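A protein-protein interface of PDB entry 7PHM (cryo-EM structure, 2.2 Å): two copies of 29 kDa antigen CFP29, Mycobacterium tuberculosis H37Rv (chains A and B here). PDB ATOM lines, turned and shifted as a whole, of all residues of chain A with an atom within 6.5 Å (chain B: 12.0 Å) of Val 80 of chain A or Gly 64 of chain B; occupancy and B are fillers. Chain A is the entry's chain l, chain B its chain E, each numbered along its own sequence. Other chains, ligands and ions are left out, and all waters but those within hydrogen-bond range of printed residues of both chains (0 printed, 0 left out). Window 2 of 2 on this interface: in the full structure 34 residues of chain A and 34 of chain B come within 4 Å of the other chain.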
ATOM      1  N   LEU A  78      -1.266  -3.714 -15.610  1.00  0.00           N
ATOM      2  CA  LEU A  78      -0.211  -3.200 -14.739  1.00  0.00           C
ATOM      3  C   LEU A  78      -0.384  -1.695 -14.632  1.00  0.00           C
ATOM      4  O   LEU A  78      -0.278  -0.996 -15.633  1.00  0.00           O
ATOM      5  CB  LEU A  78       1.161  -3.553 -15.296  1.00  0.00           C
ATOM      6  CG  LEU A  78       1.458  -5.041 -15.399  1.00  0.00           C
ATOM      7  CD1 LEU A  78       2.680  -5.259 -16.250  1.00  0.00           C
ATOM      8  CD2 LEU A  78       1.638  -5.645 -14.026  1.00  0.00           C
ATOM      9  N   ARG A  79      -0.645  -1.197 -13.434  1.00  0.00           N
ATOM     10  CA  ARG A  79      -0.890   0.223 -13.220  1.00  0.00           C
ATOM     11  C   ARG A  79       0.142   0.810 -12.265  1.00  0.00           C
ATOM     12  O   ARG A  79       0.375   0.263 -11.186  1.00  0.00           O
ATOM     13  CB  ARG A  79      -2.300   0.461 -12.677  1.00  0.00           C
ATOM     14  CG  ARG A  79      -2.592   1.916 -12.427  1.00  0.00           C
ATOM     15  CD  ARG A  79      -3.984   2.189 -11.952  1.00  0.00           C
ATOM     16  NE  ARG A  79      -4.975   2.004 -12.994  1.00  0.00           N
ATOM     17  CZ  ARG A  79      -6.277   2.135 -12.802  1.00  0.00           C
ATOM     18  NH1 ARG A  79      -6.734   2.467 -11.608  1.00  0.00           N
ATOM     19  NH2 ARG A  79      -7.115   1.955 -13.801  1.00  0.00           N
ATOM     20  N   VAL A  80       0.743   1.927 -12.658  1.00  0.00           N
ATOM     21  CA  VAL A  80       1.694   2.633 -11.804  1.00  0.00           C
ATOM     22  C   VAL A  80       1.154   4.026 -11.507  1.00  0.00           C
ATOM     23  O   VAL A  80       1.126   4.874 -12.402  1.00  0.00           O
ATOM     24  CB  VAL A  80       3.085   2.724 -12.448  1.00  0.00           C
ATOM     25  CG1 VAL A  80       4.038   3.475 -11.534  1.00  0.00           C
ATOM     26  CG2 VAL A  80       3.622   1.350 -12.773  1.00  0.00           C
ATOM     27  N   PRO A  81       0.729   4.311 -10.285  1.00  0.00           N
ATOM     28  CA  PRO A  81       0.251   5.656  -9.961  1.00  0.00           C
ATOM     29  C   PRO A  81       1.397   6.637  -9.771  1.00  0.00           C
ATOM     30  O   PRO A  81       2.507   6.275  -9.384  1.00  0.00           O
ATOM     31  CB  PRO A  81      -0.497   5.455  -8.642  1.00  0.00           C
ATOM     32  CG  PRO A  81      -0.748   4.031  -8.559  1.00  0.00           C
ATOM     33  CD  PRO A  81       0.417   3.368  -9.208  1.00  0.00           C
ATOM     34  N   PHE A  82       1.101   7.901 -10.044  1.00  0.00           N
ATOM     35  CA  PHE A  82       2.044   8.975  -9.782  1.00  0.00           C
ATOM     36  C   PHE A  82       1.274  10.255  -9.501  1.00  0.00           C
ATOM     37  O   PHE A  82       0.141  10.431  -9.947  1.00  0.00           O
ATOM     38  CB  PHE A  82       3.045   9.155 -10.934  1.00  0.00           C
ATOM     39  CG  PHE A  82       2.438   9.580 -12.236  1.00  0.00           C
ATOM     40  CD1 PHE A  82       1.900   8.647 -13.104  1.00  0.00           C
ATOM     41  CD2 PHE A  82       2.478  10.905 -12.629  1.00  0.00           C
ATOM     42  CE1 PHE A  82       1.374   9.030 -14.305  1.00  0.00           C
ATOM     43  CE2 PHE A  82       1.943  11.292 -13.830  1.00  0.00           C
ATOM     44  CZ  PHE A  82       1.399  10.356 -14.672  1.00  0.00           C
ATOM     45  N   GLU A 106       9.570   8.748 -13.017  1.00  0.00           N
ATOM     46  CA  GLU A 106       9.670   7.618 -12.104  1.00  0.00           C
ATOM     47  C   GLU A 106       8.610   6.569 -12.406  1.00  0.00           C
ATOM     48  O   GLU A 106       8.889   5.371 -12.340  1.00  0.00           O
ATOM     49  CB  GLU A 106       9.541   8.076 -10.657  1.00  0.00           C
ATOM     50  CG  GLU A 106      10.669   8.921 -10.154  1.00  0.00           C
ATOM     51  CD  GLU A 106      10.475   9.336  -8.709  1.00  0.00           C
ATOM     52  OE1 GLU A 106       9.416   9.003  -8.130  1.00  0.00           O
ATOM     53  OE2 GLU A 106      11.372  10.007  -8.157  1.00  0.00           O
ATOM     54  N   ALA A 107       7.401   7.002 -12.765  1.00  0.00           N
ATOM     55  CA  ALA A 107       6.343   6.052 -13.079  1.00  0.00           C
ATOM     56  C   ALA A 107       6.603   5.348 -14.404  1.00  0.00           C
ATOM     57  O   ALA A 107       6.313   4.158 -14.537  1.00  0.00           O
ATOM     58  CB  ALA A 107       4.988   6.753 -13.096  1.00  0.00           C
ATOM     59  N   ALA A 108       7.161   6.057 -15.386  1.00  0.00           N
ATOM     60  CA  ALA A 108       7.472   5.429 -16.664  1.00  0.00           C
ATOM     61  C   ALA A 108       8.632   4.460 -16.535  1.00  0.00           C
ATOM     62  O   ALA A 108       8.636   3.407 -17.173  1.00  0.00           O
ATOM     63  CB  ALA A 108       7.754   6.488 -17.723  1.00  0.00           C
ATOM     64  N   LYS A 110       9.292   2.876 -13.700  1.00  0.00           N
ATOM     65  CA  LYS A 110       8.721   1.771 -12.942  1.00  0.00           C
ATOM     66  C   LYS A 110       7.908   0.847 -13.839  1.00  0.00           C
ATOM     67  O   LYS A 110       8.001  -0.375 -13.717  1.00  0.00           O
ATOM     68  CB  LYS A 110       7.854   2.314 -11.812  1.00  0.00           C
ATOM     69  CG  LYS A 110       7.165   1.271 -10.987  1.00  0.00           C
ATOM     70  CD  LYS A 110       8.115   0.525 -10.096  1.00  0.00           C
ATOM     71  CE  LYS A 110       8.521   1.385  -8.913  1.00  0.00           C
ATOM     72  NZ  LYS A 110       9.402   0.633  -7.983  1.00  0.00           N
ATOM     73  N   LEU A 111       7.126   1.414 -14.756  1.00  0.00           N
ATOM     74  CA  LEU A 111       6.322   0.593 -15.652  1.00  0.00           C
ATOM     75  C   LEU A 111       7.193  -0.121 -16.672  1.00  0.00           C
ATOM     76  O   LEU A 111       6.906  -1.262 -17.042  1.00  0.00           O
ATOM     77  CB  LEU A 111       5.266   1.444 -16.352  1.00  0.00           C
ATOM     78  CG  LEU A 111       4.300   0.731 -17.300  1.00  0.00           C
ATOM     79  CD1 LEU A 111       3.504  -0.302 -16.554  1.00  0.00           C
ATOM     80  CD2 LEU A 111       3.382   1.717 -17.971  1.00  0.00           C
ATOM     81  N   ALA A 112       8.273   0.523 -17.115  1.00  0.00           N
ATOM     82  CA  ALA A 112       9.187  -0.133 -18.039  1.00  0.00           C
ATOM     83  C   ALA A 112       9.934  -1.269 -17.364  1.00  0.00           C
ATOM     84  O   ALA A 112      10.200  -2.288 -18.001  1.00  0.00           O
ATOM     85  CB  ALA A 112      10.173   0.867 -18.635  1.00  0.00           C
ATOM     86  N   VAL A 114       8.808  -3.187 -14.826  1.00  0.00           N
ATOM     87  CA  VAL A 114       7.874  -4.281 -14.579  1.00  0.00           C
ATOM     88  C   VAL A 114       7.611  -5.067 -15.854  1.00  0.00           C
ATOM     89  O   VAL A 114       7.585  -6.297 -15.831  1.00  0.00           O
ATOM     90  CB  VAL A 114       6.577  -3.736 -13.957  1.00  0.00           C
ATOM     91  CG1 VAL A 114       5.518  -4.795 -13.885  1.00  0.00           C
ATOM     92  CG2 VAL A 114       6.872  -3.289 -12.586  1.00  0.00           C
ATOM     93  N   LEU A 244      -2.466  10.699 -10.942  1.00  0.00           N
ATOM     94  CA  LEU A 244      -2.580  10.079 -12.245  1.00  0.00           C
ATOM     95  C   LEU A 244      -2.024   8.666 -12.172  1.00  0.00           C
ATOM     96  O   LEU A 244      -1.588   8.205 -11.122  1.00  0.00           O
ATOM     97  CB  LEU A 244      -1.846  10.901 -13.305  1.00  0.00           C
ATOM     98  CG  LEU A 244      -2.302  12.331 -13.585  1.00  0.00           C
ATOM     99  CD1 LEU A 244      -1.357  12.976 -14.562  1.00  0.00           C
ATOM    100  CD2 LEU A 244      -3.711  12.377 -14.106  1.00  0.00           C
ATOM    101  N   TYR A 245      -2.040   7.977 -13.304  1.00  0.00           N
ATOM    102  CA  TYR A 245      -1.414   6.669 -13.389  1.00  0.00           C
ATOM    103  C   TYR A 245      -0.996   6.398 -14.820  1.00  0.00           C
ATOM    104  O   TYR A 245      -1.554   6.955 -15.763  1.00  0.00           O
ATOM    105  CB  TYR A 245      -2.325   5.536 -12.880  1.00  0.00           C
ATOM    106  CG  TYR A 245      -3.683   5.441 -13.541  1.00  0.00           C
ATOM    107  CD1 TYR A 245      -4.783   6.072 -12.984  1.00  0.00           C
ATOM    108  CD2 TYR A 245      -3.868   4.722 -14.717  1.00  0.00           C
ATOM    109  CE1 TYR A 245      -6.015   5.998 -13.572  1.00  0.00           C
ATOM    110  CE2 TYR A 245      -5.097   4.653 -15.317  1.00  0.00           C
ATOM    111  CZ  TYR A 245      -6.168   5.286 -14.735  1.00  0.00           C
ATOM    112  OH  TYR A 245      -7.392   5.223 -15.326  1.00  0.00           O
ATOM    113  N   LEU A 246      -0.008   5.538 -14.965  1.00  0.00           N
ATOM    114  CA  LEU A 246       0.301   4.912 -16.236  1.00  0.00           C
ATOM    115  C   LEU A 246      -0.194   3.484 -16.174  1.00  0.00           C
ATOM    116  O   LEU A 246      -0.067   2.833 -15.138  1.00  0.00           O
ATOM    117  CB  LEU A 246       1.794   4.893 -16.497  1.00  0.00           C
ATOM    118  CG  LEU A 246       2.533   6.200 -16.397  1.00  0.00           C
ATOM    119  CD1 LEU A 246       3.908   5.852 -16.687  1.00  0.00           C
ATOM    120  CD2 LEU A 246       2.045   7.167 -17.396  1.00  0.00           C
ATOM    121  N   GLN A 247      -0.743   2.991 -17.273  1.00  0.00           N
ATOM    122  CA  GLN A 247      -1.131   1.595 -17.251  1.00  0.00           C
ATOM    123  C   GLN A 247      -1.020   0.975 -18.630  1.00  0.00           C
ATOM    124  O   GLN A 247      -1.094   1.657 -19.651  1.00  0.00           O
ATOM    125  CB  GLN A 247      -2.544   1.384 -16.704  1.00  0.00           C
ATOM    126  CG  GLN A 247      -3.647   1.779 -17.608  1.00  0.00           C
ATOM    127  CD  GLN A 247      -4.996   1.534 -16.983  1.00  0.00           C
ATOM    128  OE1 GLN A 247      -5.092   1.123 -15.837  1.00  0.00           O
ATOM    129  NE2 GLN A 247      -6.043   1.772 -17.742  1.00  0.00           N
ATOM    130  N   VAL B  58      -4.362  -9.497  -7.973  1.00  0.00           N
ATOM    131  CA  VAL B  58      -3.215 -10.379  -8.039  1.00  0.00           C
ATOM    132  C   VAL B  58      -2.058  -9.643  -7.386  1.00  0.00           C
ATOM    133  O   VAL B  58      -2.036  -8.411  -7.344  1.00  0.00           O
ATOM    134  CB  VAL B  58      -2.933 -10.798  -9.508  1.00  0.00           C
ATOM    135  CG1 VAL B  58      -2.384  -9.667 -10.335  1.00  0.00           C
ATOM    136  CG2 VAL B  58      -2.077 -11.998  -9.578  1.00  0.00           C
ATOM    137  N   LYS B  59      -1.134 -10.403  -6.807  1.00  0.00           N
ATOM    138  CA  LYS B  59      -0.022  -9.807  -6.087  1.00  0.00           C
ATOM    139  C   LYS B  59       0.887  -9.052  -7.043  1.00  0.00           C
ATOM    140  O   LYS B  59       1.207  -9.537  -8.127  1.00  0.00           O
ATOM    141  CB  LYS B  59       0.772 -10.878  -5.351  1.00  0.00           C
ATOM    142  CG  LYS B  59       1.864 -10.307  -4.485  1.00  0.00           C
ATOM    143  CD  LYS B  59       2.617 -11.367  -3.722  1.00  0.00           C
ATOM    144  CE  LYS B  59       3.692 -10.726  -2.861  1.00  0.00           C
ATOM    145  NZ  LYS B  59       4.434 -11.729  -2.053  1.00  0.00           N
ATOM    146  N   ALA B  60       1.266  -7.851  -6.640  1.00  0.00           N
ATOM    147  CA  ALA B  60       2.070  -6.991  -7.483  1.00  0.00           C
ATOM    148  C   ALA B  60       3.484  -7.543  -7.618  1.00  0.00           C
ATOM    149  O   ALA B  60       4.020  -8.125  -6.669  1.00  0.00           O
ATOM    150  CB  ALA B  60       2.114  -5.591  -6.889  1.00  0.00           C
ATOM    151  N   PRO B  61       4.117  -7.379  -8.777  1.00  0.00           N
ATOM    152  CA  PRO B  61       5.500  -7.842  -8.921  1.00  0.00           C
ATOM    153  C   PRO B  61       6.514  -6.932  -8.249  1.00  0.00           C
ATOM    154  O   PRO B  61       7.604  -7.396  -7.901  1.00  0.00           O
ATOM    155  CB  PRO B  61       5.681  -7.886 -10.443  1.00  0.00           C
ATOM    156  CG  PRO B  61       4.747  -6.880 -10.943  1.00  0.00           C
ATOM    157  CD  PRO B  61       3.579  -6.839 -10.035  1.00  0.00           C
ATOM    158  N   THR B  62       6.187  -5.659  -8.045  1.00  0.00           N
ATOM    159  CA  THR B  62       7.070  -4.679  -7.425  1.00  0.00           C
ATOM    160  C   THR B  62       6.167  -3.713  -6.667  1.00  0.00           C
ATOM    161  O   THR B  62       4.994  -3.565  -7.012  1.00  0.00           O
ATOM    162  CB  THR B  62       7.922  -3.948  -8.488  1.00  0.00           C
ATOM    163  OG1 THR B  62       8.558  -4.908  -9.334  1.00  0.00           O
ATOM    164  CG2 THR B  62       9.034  -3.114  -7.876  1.00  0.00           C
ATOM    165  N   ASN B  63       6.696  -3.079  -5.619  1.00  0.00           N
ATOM    166  CA  ASN B  63       5.937  -2.037  -4.937  1.00  0.00           C
ATOM    167  C   ASN B  63       5.757  -0.817  -5.838  1.00  0.00           C
ATOM    168  O   ASN B  63       6.539  -0.573  -6.757  1.00  0.00           O
ATOM    169  CB  ASN B  63       6.602  -1.659  -3.609  1.00  0.00           C
ATOM    170  CG  ASN B  63       8.057  -1.228  -3.752  1.00  0.00           C
ATOM    171  OD1 ASN B  63       8.605  -1.121  -4.847  1.00  0.00           O
ATOM    172  ND2 ASN B  63       8.695  -0.990  -2.614  1.00  0.00           N
ATOM    173  N   GLY B  64       4.683  -0.073  -5.596  1.00  0.00           N
ATOM    174  CA  GLY B  64       4.324   1.025  -6.464  1.00  0.00           C
ATOM    175  C   GLY B  64       3.617   0.623  -7.735  1.00  0.00           C
ATOM    176  O   GLY B  64       3.347   1.484  -8.575  1.00  0.00           O
ATOM    177  N   VAL B  65       3.338  -0.661  -7.917  1.00  0.00           N
ATOM    178  CA  VAL B  65       2.630  -1.171  -9.082  1.00  0.00           C
ATOM    179  C   VAL B  65       1.375  -1.851  -8.572  1.00  0.00           C
ATOM    180  O   VAL B  65       1.411  -2.526  -7.545  1.00  0.00           O
ATOM    181  CB  VAL B  65       3.507  -2.142  -9.893  1.00  0.00           C
ATOM    182  CG1 VAL B  65       2.779  -2.676 -11.111  1.00  0.00           C
ATOM    183  CG2 VAL B  65       4.760  -1.450 -10.302  1.00  0.00           C
ATOM    184  N   ILE B  66       0.259  -1.618  -9.239  1.00  0.00           N
ATOM    185  CA  ILE B  66      -0.979  -2.322  -8.946  1.00  0.00           C
ATOM    186  C   ILE B  66      -1.265  -3.230 -10.124  1.00  0.00           C
ATOM    187  O   ILE B  66      -1.306  -2.774 -11.271  1.00  0.00           O
ATOM    188  CB  ILE B  66      -2.142  -1.360  -8.664  1.00  0.00           C
ATOM    189  CG1 ILE B  66      -1.967  -0.694  -7.303  1.00  0.00           C
ATOM    190  CG2 ILE B  66      -3.447  -2.078  -8.675  1.00  0.00           C
ATOM    191  CD1 ILE B  66      -1.325   0.625  -7.344  1.00  0.00           C
ATOM    192  N   ALA B  67      -1.431  -4.513  -9.850  1.00  0.00           N
ATOM    193  CA  ALA B  67      -1.630  -5.501 -10.892  1.00  0.00           C
ATOM    194  C   ALA B  67      -2.999  -6.148 -10.759  1.00  0.00           C
ATOM    195  O   ALA B  67      -3.458  -6.439  -9.655  1.00  0.00           O
ATOM    196  CB  ALA B  67      -0.527  -6.553 -10.860  1.00  0.00           C
ATOM    197  N   HIS B  68      -3.651  -6.348 -11.895  1.00  0.00           N
ATOM    198  CA  HIS B  68      -4.908  -7.075 -11.972  1.00  0.00           C
ATOM    199  C   HIS B  68      -4.879  -8.031 -13.148  1.00  0.00           C
ATOM    200  O   HIS B  68      -4.522  -7.646 -14.260  1.00  0.00           O
ATOM    201  CB  HIS B  68      -6.114  -6.149 -12.144  1.00  0.00           C
ATOM    202  CG  HIS B  68      -6.460  -5.373 -10.923  1.00  0.00           C
ATOM    203  ND1 HIS B  68      -5.957  -4.117 -10.671  1.00  0.00           N
ATOM    204  CD2 HIS B  68      -7.255  -5.677  -9.876  1.00  0.00           C
ATOM    205  CE1 HIS B  68      -6.434  -3.678  -9.525  1.00  0.00           C
ATOM    206  NE2 HIS B  68      -7.222  -4.606  -9.021  1.00  0.00           N
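Printed residues of chain A that touch a printed residue of chain B: Leu 78, Arg 79, Val 80, Pro 81, Lys 110 and Val 114. Along chain A the printed residues that touch a printed residue of chain B span positions 78 to 114. Of the 11 printed residues of chain B, 7 touch a printed residue of chain A. Among the printed residues, 13 pairs touch across the chains. Among the printed residues, no Asp or Glu carboxylate lies within 4 Å of a Lys or Arg side-chain nitrogen of the other chain.
Printed residues of chain B within 4 Å of Val 80 of chain A: Gly 64 (3.6 Å) and Val 65 (3.9 Å). Gly 64 of chain B touches just these residues of chain A: Val 80 (3.6 Å) and Pro 81 (3.5 Å). Of the printed residues of chain B, Leu 78 of chain A touches Ile 66 and Ala 67. No residue of chain B comes within 4 Å of Phe 82 of chain A. No residue of chain B comes within 4 Å of Ala 107 of chain A. No residue of chain B comes within 4 Å of Ala 108 of chain A. Of chain B, only Thr 62 (3.8 Å), Asn 63 (3.3 Å) and Val 65 (3.7 Å) come within 4 Å of Lys 110 of chain A. Leu 111 of chain A touches none of the printed residues of chain B. No residue of chain B comes within 4 Å of Leu 246 of chain A. Of the printed residues of chain A, Ile 66 of chain B touches Leu 78, Arg 79 and Pro 81. Printed residues of chain A within 4 Å of Ala 67 of chain B: Leu 78 (3.9 Å). Of the printed residues of chain A, Thr 62 of chain B touches Lys 110. Of the printed residues of chain A, Pro 61 of chain B touches Val 114 (3.7 Å). His 68 of chain B touches none of the printed residues of chain A. Val 58 of chain B touches none of the printed residues of chain A.
The backbone carbonyl oxygen of Asn 63 of chain B sits at hydrogen-bond distance from the side-chain amino group of Lys 110 of chain A. The backbone carbonyl oxygen of Arg 79 of chain A sits at hydrogen-bond distance from the backbone NH of Ile 66 of chain B (2.7 Å).
Leu 78 of chain A touches Ile 66 of chain B (C to O, 3.6 Å). Val 65 of chain B touches Arg 79 of chain A (CA to O, 3.4 Å). Val 80 of chain A touches Gly 64 of chain B (CG1 to O, 3.6 Å). CG2 of Val 80 of chain A touches CG2 of Val 65 of chain B, at 3.9 Å. CD of Pro 81 of chain A touches O of Gly 64 of chain B, 3.5 Å away. Ile 66 of chain B touches Pro 81 of chain A. NZ of Lys 110 of chain A touches CG2 of Thr 62 of chain B (3.8 Å). Val 65 of chain B touches Lys 110 of chain A. Pro 61 of chain B touches Val 114 of chain A. CG2 of Val 65 of chain B touches CG2 of Val 114 of chain A (3.6 Å).
No position is printed for both chains.
NE of Arg 79 of chain A sits at hydrogen-bond distance from OE1 of Gln 247 of chain A (3.0 Å). O of Leu 246 of chain A sits at hydrogen-bond distance from N of Val 80 of chain A (2.8 Å).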
